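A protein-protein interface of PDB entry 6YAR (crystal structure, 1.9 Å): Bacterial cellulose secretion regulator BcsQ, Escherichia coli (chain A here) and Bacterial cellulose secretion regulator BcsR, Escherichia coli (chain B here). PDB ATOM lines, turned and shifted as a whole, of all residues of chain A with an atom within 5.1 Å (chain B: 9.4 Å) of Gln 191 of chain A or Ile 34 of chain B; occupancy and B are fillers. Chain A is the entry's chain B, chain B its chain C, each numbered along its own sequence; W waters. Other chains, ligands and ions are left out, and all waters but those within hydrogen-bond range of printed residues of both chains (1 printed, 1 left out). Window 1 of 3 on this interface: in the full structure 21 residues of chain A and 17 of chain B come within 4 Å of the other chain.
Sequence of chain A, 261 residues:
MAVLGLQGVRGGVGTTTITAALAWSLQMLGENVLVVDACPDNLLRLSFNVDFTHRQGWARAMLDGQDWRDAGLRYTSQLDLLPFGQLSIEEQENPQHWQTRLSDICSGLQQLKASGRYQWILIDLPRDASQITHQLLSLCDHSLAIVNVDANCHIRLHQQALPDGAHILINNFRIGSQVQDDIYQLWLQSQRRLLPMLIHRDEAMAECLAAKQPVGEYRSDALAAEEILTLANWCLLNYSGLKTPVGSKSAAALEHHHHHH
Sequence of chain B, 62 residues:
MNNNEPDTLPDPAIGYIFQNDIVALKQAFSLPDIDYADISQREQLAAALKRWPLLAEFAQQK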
ATOM      1  N   LEU A 157     -13.750  23.795  -9.029  1.00  0.00           N
ATOM      2  CA  LEU A 157     -14.845  23.016  -9.608  1.00  0.00           C
ATOM      3  C   LEU A 157     -16.220  23.503  -9.167  1.00  0.00           C
ATOM      4  O   LEU A 157     -17.224  23.084  -9.760  1.00  0.00           O
ATOM      5  CB  LEU A 157     -14.695  21.526  -9.251  1.00  0.00           C
ATOM      6  CG  LEU A 157     -13.563  20.721  -9.906  1.00  0.00           C
ATOM      7  CD1 LEU A 157     -13.496  19.272  -9.352  1.00  0.00           C
ATOM      8  CD2 LEU A 157     -13.689  20.713 -11.430  1.00  0.00           C
ATOM      9  N   HIS A 158     -16.295  24.361  -8.146  1.00  0.00           N
ATOM     10  CA  HIS A 158     -17.556  24.934  -7.693  1.00  0.00           C
ATOM     11  C   HIS A 158     -17.798  26.343  -8.212  1.00  0.00           C
ATOM     12  O   HIS A 158     -18.890  26.876  -8.000  1.00  0.00           O
ATOM     13  CB  HIS A 158     -17.619  24.969  -6.161  1.00  0.00           C
ATOM     14  CG  HIS A 158     -17.594  23.615  -5.520  1.00  0.00           C
ATOM     15  ND1 HIS A 158     -16.428  22.907  -5.325  1.00  0.00           N
ATOM     16  CD2 HIS A 158     -18.592  22.842  -5.029  1.00  0.00           C
ATOM     17  CE1 HIS A 158     -16.710  21.754  -4.744  1.00  0.00           C
ATOM     18  NE2 HIS A 158     -18.015  21.693  -4.548  1.00  0.00           N
ATOM     19  N   ILE A 168     -13.692  14.896 -16.279  1.00  0.00           N
ATOM     20  CA  ILE A 168     -12.636  15.328 -15.375  1.00  0.00           C
ATOM     21  C   ILE A 168     -11.641  14.187 -15.206  1.00  0.00           C
ATOM     22  O   ILE A 168     -12.032  13.053 -14.898  1.00  0.00           O
ATOM     23  CB  ILE A 168     -13.220  15.767 -14.018  1.00  0.00           C
ATOM     24  CG1 ILE A 168     -14.148  16.970 -14.207  1.00  0.00           C
ATOM     25  CG2 ILE A 168     -12.117  16.088 -13.049  1.00  0.00           C
ATOM     26  CD1 ILE A 168     -14.953  17.328 -12.949  1.00  0.00           C
ATOM     27  N   LEU A 186     -14.844  12.197  -1.429  1.00  0.00           N
ATOM     28  CA  LEU A 186     -15.974  13.091  -1.649  1.00  0.00           C
ATOM     29  C   LEU A 186     -16.303  13.211  -3.134  1.00  0.00           C
ATOM     30  O   LEU A 186     -17.474  13.153  -3.528  1.00  0.00           O
ATOM     31  CB  LEU A 186     -15.664  14.463  -1.048  1.00  0.00           C
ATOM     32  CG  LEU A 186     -16.758  15.531  -1.060  1.00  0.00           C
ATOM     33  CD1 LEU A 186     -17.992  15.021  -0.348  1.00  0.00           C
ATOM     34  CD2 LEU A 186     -16.259  16.812  -0.392  1.00  0.00           C
ATOM     35  N   TRP A 187     -15.281  13.398  -3.974  1.00  0.00           N
ATOM     36  CA  TRP A 187     -15.508  13.482  -5.417  1.00  0.00           C
ATOM     37  C   TRP A 187     -16.177  12.217  -5.956  1.00  0.00           C
ATOM     38  O   TRP A 187     -17.018  12.286  -6.865  1.00  0.00           O
ATOM     39  CB  TRP A 187     -14.189  13.714  -6.156  1.00  0.00           C
ATOM     40  CG  TRP A 187     -13.617  15.092  -6.061  1.00  0.00           C
ATOM     41  CD1 TRP A 187     -14.084  16.135  -5.308  1.00  0.00           C
ATOM     42  CD2 TRP A 187     -12.469  15.588  -6.769  1.00  0.00           C
ATOM     43  NE1 TRP A 187     -13.292  17.249  -5.504  1.00  0.00           N
ATOM     44  CE2 TRP A 187     -12.292  16.938  -6.390  1.00  0.00           C
ATOM     45  CE3 TRP A 187     -11.574  15.018  -7.689  1.00  0.00           C
ATOM     46  CZ2 TRP A 187     -11.247  17.728  -6.893  1.00  0.00           C
ATOM     47  CZ3 TRP A 187     -10.539  15.791  -8.182  1.00  0.00           C
ATOM     48  CH2 TRP A 187     -10.389  17.144  -7.794  1.00  0.00           C
ATOM     49  N   LEU A 188     -15.794  11.050  -5.428  1.00  0.00           N
ATOM     50  CA  LEU A 188     -16.350   9.801  -5.932  1.00  0.00           C
ATOM     51  C   LEU A 188     -17.861   9.759  -5.765  1.00  0.00           C
ATOM     52  O   LEU A 188     -18.554   9.108  -6.553  1.00  0.00           O
ATOM     53  CB  LEU A 188     -15.711   8.600  -5.222  1.00  0.00           C
ATOM     54  CG  LEU A 188     -14.275   8.210  -5.574  1.00  0.00           C
ATOM     55  CD1 LEU A 188     -13.827   7.026  -4.716  1.00  0.00           C
ATOM     56  CD2 LEU A 188     -14.159   7.880  -7.053  1.00  0.00           C
ATOM     57  N   GLN A 189     -18.391  10.455  -4.759  1.00  0.00           N
ATOM     58  CA  GLN A 189     -19.822  10.451  -4.500  1.00  0.00           C
ATOM     59  C   GLN A 189     -20.552  11.645  -5.100  1.00  0.00           C
ATOM     60  O   GLN A 189     -21.788  11.626  -5.142  1.00  0.00           O
ATOM     61  CB  GLN A 189     -20.084  10.407  -2.988  1.00  0.00           C
ATOM     62  CG  GLN A 189     -19.596   9.131  -2.310  1.00  0.00           C
ATOM     63  CD  GLN A 189     -20.442   7.921  -2.677  1.00  0.00           C
ATOM     64  OE1 GLN A 189     -21.611   7.836  -2.295  1.00  0.00           O
ATOM     65  NE2 GLN A 189     -19.859   6.985  -3.424  1.00  0.00           N
ATOM     66  N   SER A 190     -19.834  12.668  -5.583  1.00  0.00           N
ATOM     67  CA  SER A 190     -20.477  13.933  -5.922  1.00  0.00           C
ATOM     68  C   SER A 190     -20.131  14.468  -7.310  1.00  0.00           C
ATOM     69  O   SER A 190     -20.945  15.165  -7.922  1.00  0.00           O
ATOM     70  CB  SER A 190     -20.126  14.989  -4.873  1.00  0.00           C
ATOM     71  OG  SER A 190     -18.723  15.177  -4.780  1.00  0.00           O
ATOM     72  N   GLN A 191     -18.934  14.172  -7.814  1.00  0.00           N
ATOM     73  CA  GLN A 191     -18.472  14.727  -9.087  1.00  0.00           C
ATOM     74  C   GLN A 191     -18.943  13.820 -10.222  1.00  0.00           C
ATOM     75  O   GLN A 191     -18.313  12.801 -10.526  1.00  0.00           O
ATOM     76  CB  GLN A 191     -16.956  14.885  -9.086  1.00  0.00           C
ATOM     77  CG  GLN A 191     -16.434  15.926  -8.109  1.00  0.00           C
ATOM     78  CD  GLN A 191     -16.801  17.368  -8.483  1.00  0.00           C
ATOM     79  OE1 GLN A 191     -16.897  18.233  -7.610  1.00  0.00           O
ATOM     80  NE2 GLN A 191     -16.994  17.628  -9.771  1.00  0.00           N
ATOM     81  N   ARG A 192     -20.040  14.220 -10.878  1.00  0.00           N
ATOM     82  CA  ARG A 192     -20.714  13.350 -11.838  1.00  0.00           C
ATOM     83  C   ARG A 192     -19.884  13.115 -13.095  1.00  0.00           C
ATOM     84  O   ARG A 192     -20.070  12.094 -13.771  1.00  0.00           O
ATOM     85  CB  ARG A 192     -22.075  13.943 -12.219  1.00  0.00           C
ATOM     86  CG  ARG A 192     -23.001  14.209 -11.036  1.00  0.00           C
ATOM     87  CD  ARG A 192     -24.125  13.186 -10.953  1.00  0.00           C
ATOM     88  NE  ARG A 192     -25.189  13.455 -11.920  1.00  0.00           N
ATOM     89  CZ  ARG A 192     -26.334  14.065 -11.625  1.00  0.00           C
ATOM     90  NH1 ARG A 192     -26.576  14.470 -10.386  1.00  0.00           N
ATOM     91  NH2 ARG A 192     -27.242  14.266 -12.571  1.00  0.00           N
ATOM     92  N   ARG A 193     -18.976  14.031 -13.441  1.00  0.00           N
ATOM     93  CA  ARG A 193     -18.253  13.911 -14.700  1.00  0.00           C
ATOM     94  C   ARG A 193     -16.824  13.417 -14.510  1.00  0.00           C
ATOM     95  O   ARG A 193     -16.010  13.507 -15.440  1.00  0.00           O
ATOM     96  CB  ARG A 193     -18.292  15.239 -15.451  1.00  0.00           C
ATOM     97  CG  ARG A 193     -19.729  15.689 -15.699  1.00  0.00           C
ATOM     98  CD  ARG A 193     -19.866  16.547 -16.932  1.00  0.00           C
ATOM     99  NE  ARG A 193     -19.517  15.820 -18.151  1.00  0.00           N
ATOM    100  CZ  ARG A 193     -20.373  15.090 -18.856  1.00  0.00           C
ATOM    101  NH1 ARG A 193     -21.636  14.982 -18.462  1.00  0.00           N
ATOM    102  NH2 ARG A 193     -19.967  14.471 -19.960  1.00  0.00           N
ATOM    103  N   LEU A 194     -16.520  12.865 -13.337  1.00  0.00           N
ATOM    104  CA  LEU A 194     -15.200  12.320 -13.067  1.00  0.00           C
ATOM    105  C   LEU A 194     -14.990  11.015 -13.839  1.00  0.00           C
ATOM    106  O   LEU A 194     -15.868  10.149 -13.864  1.00  0.00           O
ATOM    107  CB  LEU A 194     -15.047  12.087 -11.559  1.00  0.00           C
ATOM    108  CG  LEU A 194     -13.682  11.693 -10.995  1.00  0.00           C
ATOM    109  CD1 LEU A 194     -12.696  12.829 -11.166  1.00  0.00           C
ATOM    110  CD2 LEU A 194     -13.785  11.260  -9.515  1.00  0.00           C
ATOM    111  N   SER B  30     -20.081  25.671 -18.827  1.00  0.00           N
ATOM    112  CA  SER B  30     -21.014  25.566 -17.719  1.00  0.00           C
ATOM    113  C   SER B  30     -20.258  25.140 -16.467  1.00  0.00           C
ATOM    114  O   SER B  30     -19.135  24.632 -16.534  1.00  0.00           O
ATOM    115  CB  SER B  30     -22.153  24.581 -18.028  1.00  0.00           C
ATOM    116  OG  SER B  30     -21.652  23.315 -18.424  1.00  0.00           O
ATOM    117  N   LEU B  31     -20.889  25.369 -15.319  1.00  0.00           N
ATOM    118  CA  LEU B  31     -20.295  24.955 -14.058  1.00  0.00           C
ATOM    119  C   LEU B  31     -20.381  23.435 -13.922  1.00  0.00           C
ATOM    120  O   LEU B  31     -21.355  22.825 -14.376  1.00  0.00           O
ATOM    121  CB  LEU B  31     -20.992  25.634 -12.877  1.00  0.00           C
ATOM    122  CG  LEU B  31     -20.958  27.167 -12.821  1.00  0.00           C
ATOM    123  CD1 LEU B  31     -22.136  27.777 -13.574  1.00  0.00           C
ATOM    124  CD2 LEU B  31     -20.923  27.656 -11.380  1.00  0.00           C
ATOM    125  N   PRO B  32     -19.377  22.801 -13.314  1.00  0.00           N
ATOM    126  CA  PRO B  32     -19.364  21.334 -13.226  1.00  0.00           C
ATOM    127  C   PRO B  32     -20.594  20.773 -12.524  1.00  0.00           C
ATOM    128  O   PRO B  32     -21.092  21.334 -11.546  1.00  0.00           O
ATOM    129  CB  PRO B  32     -18.086  21.046 -12.428  1.00  0.00           C
ATOM    130  CG  PRO B  32     -17.204  22.214 -12.730  1.00  0.00           C
ATOM    131  CD  PRO B  32     -18.121  23.395 -12.830  1.00  0.00           C
ATOM    132  N   ASP B  33     -21.083  19.650 -13.042  1.00  0.00           N
ATOM    133  CA  ASP B  33     -22.221  18.964 -12.443  1.00  0.00           C
ATOM    134  C   ASP B  33     -21.776  18.329 -11.130  1.00  0.00           C
ATOM    135  O   ASP B  33     -21.019  17.351 -11.128  1.00  0.00           O
ATOM    136  CB  ASP B  33     -22.770  17.922 -13.415  1.00  0.00           C
ATOM    137  CG  ASP B  33     -24.079  17.309 -12.946  1.00  0.00           C
ATOM    138  OD1 ASP B  33     -24.682  17.827 -11.979  1.00  0.00           O
ATOM    139  OD2 ASP B  33     -24.504  16.300 -13.541  1.00  0.00           O
ATOM    140  N   ILE B  34     -22.223  18.895 -10.009  1.00  0.00           N
ATOM    141  CA  ILE B  34     -21.875  18.400  -8.681  1.00  0.00           C
ATOM    142  C   ILE B  34     -23.163  18.146  -7.910  1.00  0.00           C
ATOM    143  O   ILE B  34     -24.021  19.032  -7.814  1.00  0.00           O
ATOM    144  CB  ILE B  34     -20.975  19.380  -7.907  1.00  0.00           C
ATOM    145  CG1 ILE B  34     -19.714  19.728  -8.706  1.00  0.00           C
ATOM    146  CG2 ILE B  34     -20.598  18.790  -6.552  1.00  0.00           C
ATOM    147  CD1 ILE B  34     -18.800  20.727  -7.993  1.00  0.00           C
ATOM    148  N   ASP B  35     -23.291  16.940  -7.355  1.00  0.00           N
ATOM    149  CA  ASP B  35     -24.482  16.514  -6.627  1.00  0.00           C
ATOM    150  C   ASP B  35     -24.069  16.084  -5.226  1.00  0.00           C
ATOM    151  O   ASP B  35     -23.348  15.093  -5.064  1.00  0.00           O
ATOM    152  CB  ASP B  35     -25.194  15.377  -7.355  1.00  0.00           C
ATOM    153  CG  ASP B  35     -26.292  14.750  -6.519  1.00  0.00           C
ATOM    154  OD1 ASP B  35     -27.058  15.507  -5.887  1.00  0.00           O
ATOM    155  OD2 ASP B  35     -26.397  13.508  -6.501  1.00  0.00           O
ATOM    156  N   TYR B  36     -24.540  16.817  -4.216  1.00  0.00           N
ATOM    157  CA  TYR B  36     -24.257  16.498  -2.825  1.00  0.00           C
ATOM    158  C   TYR B  36     -25.413  15.768  -2.140  1.00  0.00           C
ATOM    159  O   TYR B  36     -25.434  15.676  -0.907  1.00  0.00           O
ATOM    160  CB  TYR B  36     -23.893  17.770  -2.055  1.00  0.00           C
ATOM    161  CG  TYR B  36     -22.497  18.272  -2.350  1.00  0.00           C
ATOM    162  CD1 TYR B  36     -21.384  17.492  -2.058  1.00  0.00           C
ATOM    163  CD2 TYR B  36     -22.287  19.520  -2.921  1.00  0.00           C
ATOM    164  CE1 TYR B  36     -20.101  17.943  -2.320  1.00  0.00           C
ATOM    165  CE2 TYR B  36     -21.007  19.973  -3.188  1.00  0.00           C
ATOM    166  CZ  TYR B  36     -19.923  19.179  -2.883  1.00  0.00           C
ATOM    167  OH  TYR B  36     -18.648  19.609  -3.146  1.00  0.00           O
ATOM    168  N   ALA B  37     -26.357  15.225  -2.911  1.00  0.00           N
ATOM    169  CA  ALA B  37     -27.533  14.600  -2.312  1.00  0.00           C
ATOM    170  C   ALA B  37     -27.161  13.351  -1.523  1.00  0.00           C
ATOM    171  O   ALA B  37     -27.598  13.176  -0.380  1.00  0.00           O
ATOM    172  CB  ALA B  37     -28.560  14.265  -3.393  1.00  0.00           C
ATOM    173  N   ASP B  38     -26.351  12.469  -2.113  1.00  0.00           N
ATOM    174  CA  ASP B  38     -26.019  11.186  -1.504  1.00  0.00           C
ATOM    175  C   ASP B  38     -24.740  11.230  -0.669  1.00  0.00           C
ATOM    176  O   ASP B  38     -24.116  10.184  -0.456  1.00  0.00           O
ATOM    177  CB  ASP B  38     -25.909  10.101  -2.581  1.00  0.00           C
ATOM    178  CG  ASP B  38     -24.858  10.416  -3.634  1.00  0.00           C
ATOM    179  OD1 ASP B  38     -24.292  11.530  -3.607  1.00  0.00           O
ATOM    180  OD2 ASP B  38     -24.599   9.543  -4.492  1.00  0.00           O
ATOM    181  N   ILE B  39     -24.349  12.410  -0.181  1.00  0.00           N
ATOM    182  CA  ILE B  39     -23.111  12.538   0.586  1.00  0.00           C
ATOM    183  C   ILE B  39     -23.304  12.046   2.015  1.00  0.00           C
ATOM    184  O   ILE B  39     -22.605  11.137   2.480  1.00  0.00           O
ATOM    185  CB  ILE B  39     -22.612  13.994   0.563  1.00  0.00           C
ATOM    186  CG1 ILE B  39     -22.243  14.408  -0.860  1.00  0.00           C
ATOM    187  CG2 ILE B  39     -21.433  14.172   1.513  1.00  0.00           C
ATOM    188  CD1 ILE B  39     -21.174  13.557  -1.493  1.00  0.00           C
ATOM    189  N   LEU B  45     -17.285   9.807   4.559  1.00  0.00           N
ATOM    190  CA  LEU B  45     -17.452  11.183   4.114  1.00  0.00           C
ATOM    191  C   LEU B  45     -17.828  12.094   5.274  1.00  0.00           C
ATOM    192  O   LEU B  45     -17.398  13.251   5.323  1.00  0.00           O
ATOM    193  CB  LEU B  45     -18.500  11.263   3.005  1.00  0.00           C
ATOM    194  CG  LEU B  45     -17.951  11.263   1.577  1.00  0.00           C
ATOM    195  CD1 LEU B  45     -17.126  10.016   1.298  1.00  0.00           C
ATOM    196  CD2 LEU B  45     -19.079  11.397   0.568  1.00  0.00           C
ATOM    197  N   LEU B  55     -14.847  21.717   2.877  1.00  0.00           N
ATOM    198  CA  LEU B  55     -15.679  20.719   2.200  1.00  0.00           C
ATOM    199  C   LEU B  55     -17.111  20.742   2.712  1.00  0.00           C
ATOM    200  O   LEU B  55     -18.055  20.616   1.925  1.00  0.00           O
ATOM    201  CB  LEU B  55     -15.090  19.321   2.376  1.00  0.00           C
ATOM    202  CG  LEU B  55     -13.609  19.136   2.059  1.00  0.00           C
ATOM    203  CD1 LEU B  55     -13.211  17.698   2.315  1.00  0.00           C
ATOM    204  CD2 LEU B  55     -13.309  19.526   0.636  1.00  0.00           C
ATOM    205  N   PHE B  58     -19.151  23.666   0.947  1.00  0.00           N
ATOM    206  CA  PHE B  58     -19.722  23.408  -0.370  1.00  0.00           C
ATOM    207  C   PHE B  58     -20.836  22.368  -0.311  1.00  0.00           C
ATOM    208  O   PHE B  58     -21.802  22.457  -1.076  1.00  0.00           O
ATOM    209  CB  PHE B  58     -18.630  22.962  -1.341  1.00  0.00           C
ATOM    210  CG  PHE B  58     -17.654  24.048  -1.707  1.00  0.00           C
ATOM    211  CD1 PHE B  58     -18.074  25.168  -2.405  1.00  0.00           C
ATOM    212  CD2 PHE B  58     -16.316  23.939  -1.372  1.00  0.00           C
ATOM    213  CE1 PHE B  58     -17.177  26.175  -2.752  1.00  0.00           C
ATOM    214  CE2 PHE B  58     -15.409  24.937  -1.721  1.00  0.00           C
ATOM    215  CZ  PHE B  58     -15.842  26.059  -2.406  1.00  0.00           C
ATOM    216  N   ALA B  59     -20.730  21.388   0.589  1.00  0.00           N
ATOM    217  CA  ALA B  59     -21.727  20.329   0.667  1.00  0.00           C
ATOM    218  C   ALA B  59     -23.029  20.781   1.316  1.00  0.00           C
ATOM    219  O   ALA B  59     -24.073  20.172   1.061  1.00  0.00           O
ATOM    220  CB  ALA B  59     -21.162  19.129   1.429  1.00  0.00           C
HETATM  221  O   HOH W   1     -17.274  17.578  -4.672  1.00  0.00           O
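The guanidinium group of Arg 192 of chain A is in salt-bridge range of the side-chain carboxylate of Asp 33 of chain B (3.3 Å). A ring nitrogen (NE2) of His 158 of chain A sits at hydrogen-bond distance from the side-chain hydroxyl (OH) of Tyr 36 of chain B, at 2.6 Å. O of Gln 189 of chain A sits close to OD1 of Asp 38 of chain B (2.9 Å). N of Asp 35 of chain B lies within hydrogen-bond range of O of Ser 190 of chain A.
The backbone carbonyl oxygen (O) of Leu 186 of chain A sits at hydrogen-bond distance from the side-chain hydroxyl (OG) of Ser 190 of chain A, 2.7 Å away. N of Ala 37 of chain B is in hydrogen-bond range of OD1 of Asp 35 of chain B.
Among the printed residues, merely in contact across the chains: Leu 157 of chain A with Pro 32 of chain B, Leu 157 of chain A with Ile 34 of chain B, His 158 of chain A with Ile 34 of chain B, His 158 of chain A with Phe 58 of chain B, Leu 186 of chain A with Ile 39 of chain B, Leu 186 of chain A with Leu 45 of chain B, Leu 186 of chain A with Leu 55 of chain B, Gln 189 of chain A with Asp 35 of chain B, Gln 189 of chain A with Ile 39 of chain B, Gln 189 of chain A with Leu 45 of chain B, Ser 190 of chain A with Asp 33 of chain B, Ser 190 of chain A with Ile 34 of chain B, Ser 190 of chain A with Tyr 36 of chain B, Ser 190 of chain A with Ile 39 of chain B, Gln 191 of chain A with Ile 34 of chain B and Arg 192 of chain A with Asp 35 of chain B.
Of chain A, only Leu 157, His 158, Ser 190 and Gln 191 come within 4 Å of Ile 34 of chain B. No residue of chain B comes within 4 Å of Leu 194 of chain A. Of the printed residues of chain A, Asp 35 of chain B touches Gln 189, Ser 190 and Arg 192. Printed residues of chain A within 4 Å of Ile 39 of chain B: Leu 186 (3.7 Å), Gln 189 (3.7 Å) and Ser 190 (3.8 Å). Of the printed residues of chain A, Pro 32 of chain B touches Leu 157. Printed residues of chain A within 4 Å of Leu 55 of chain B: Leu 186 (3.9 Å). The nearest residue of chain B that does not touch Gln 191 of chain A is Asp 33 of chain B (4.2 Å). The nearest residue of chain A that does not touch Ile 34 of chain B is Arg 192 of chain A (4.9 Å).
Of the 12 printed residues of chain A, 7 touch a printed residue of chain B. Printed residues of chain A that touch a printed residue of chain B: Leu 157, His 158, Leu 186, Gln 189, Ser 190, Gln 191 and Arg 192. Hydrophobic or aromatic side chains of chain B that line the printed part of chain A: Pro 32, Ile 34, Tyr 36, Ile 39, Leu 45, Leu 55 and Phe 58.
Water W1 lies within hydrogen-bond range of OG of Ser 190 of chain A, OH of Tyr 36 of chain B and OE1 of Gln 191 of chain A.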
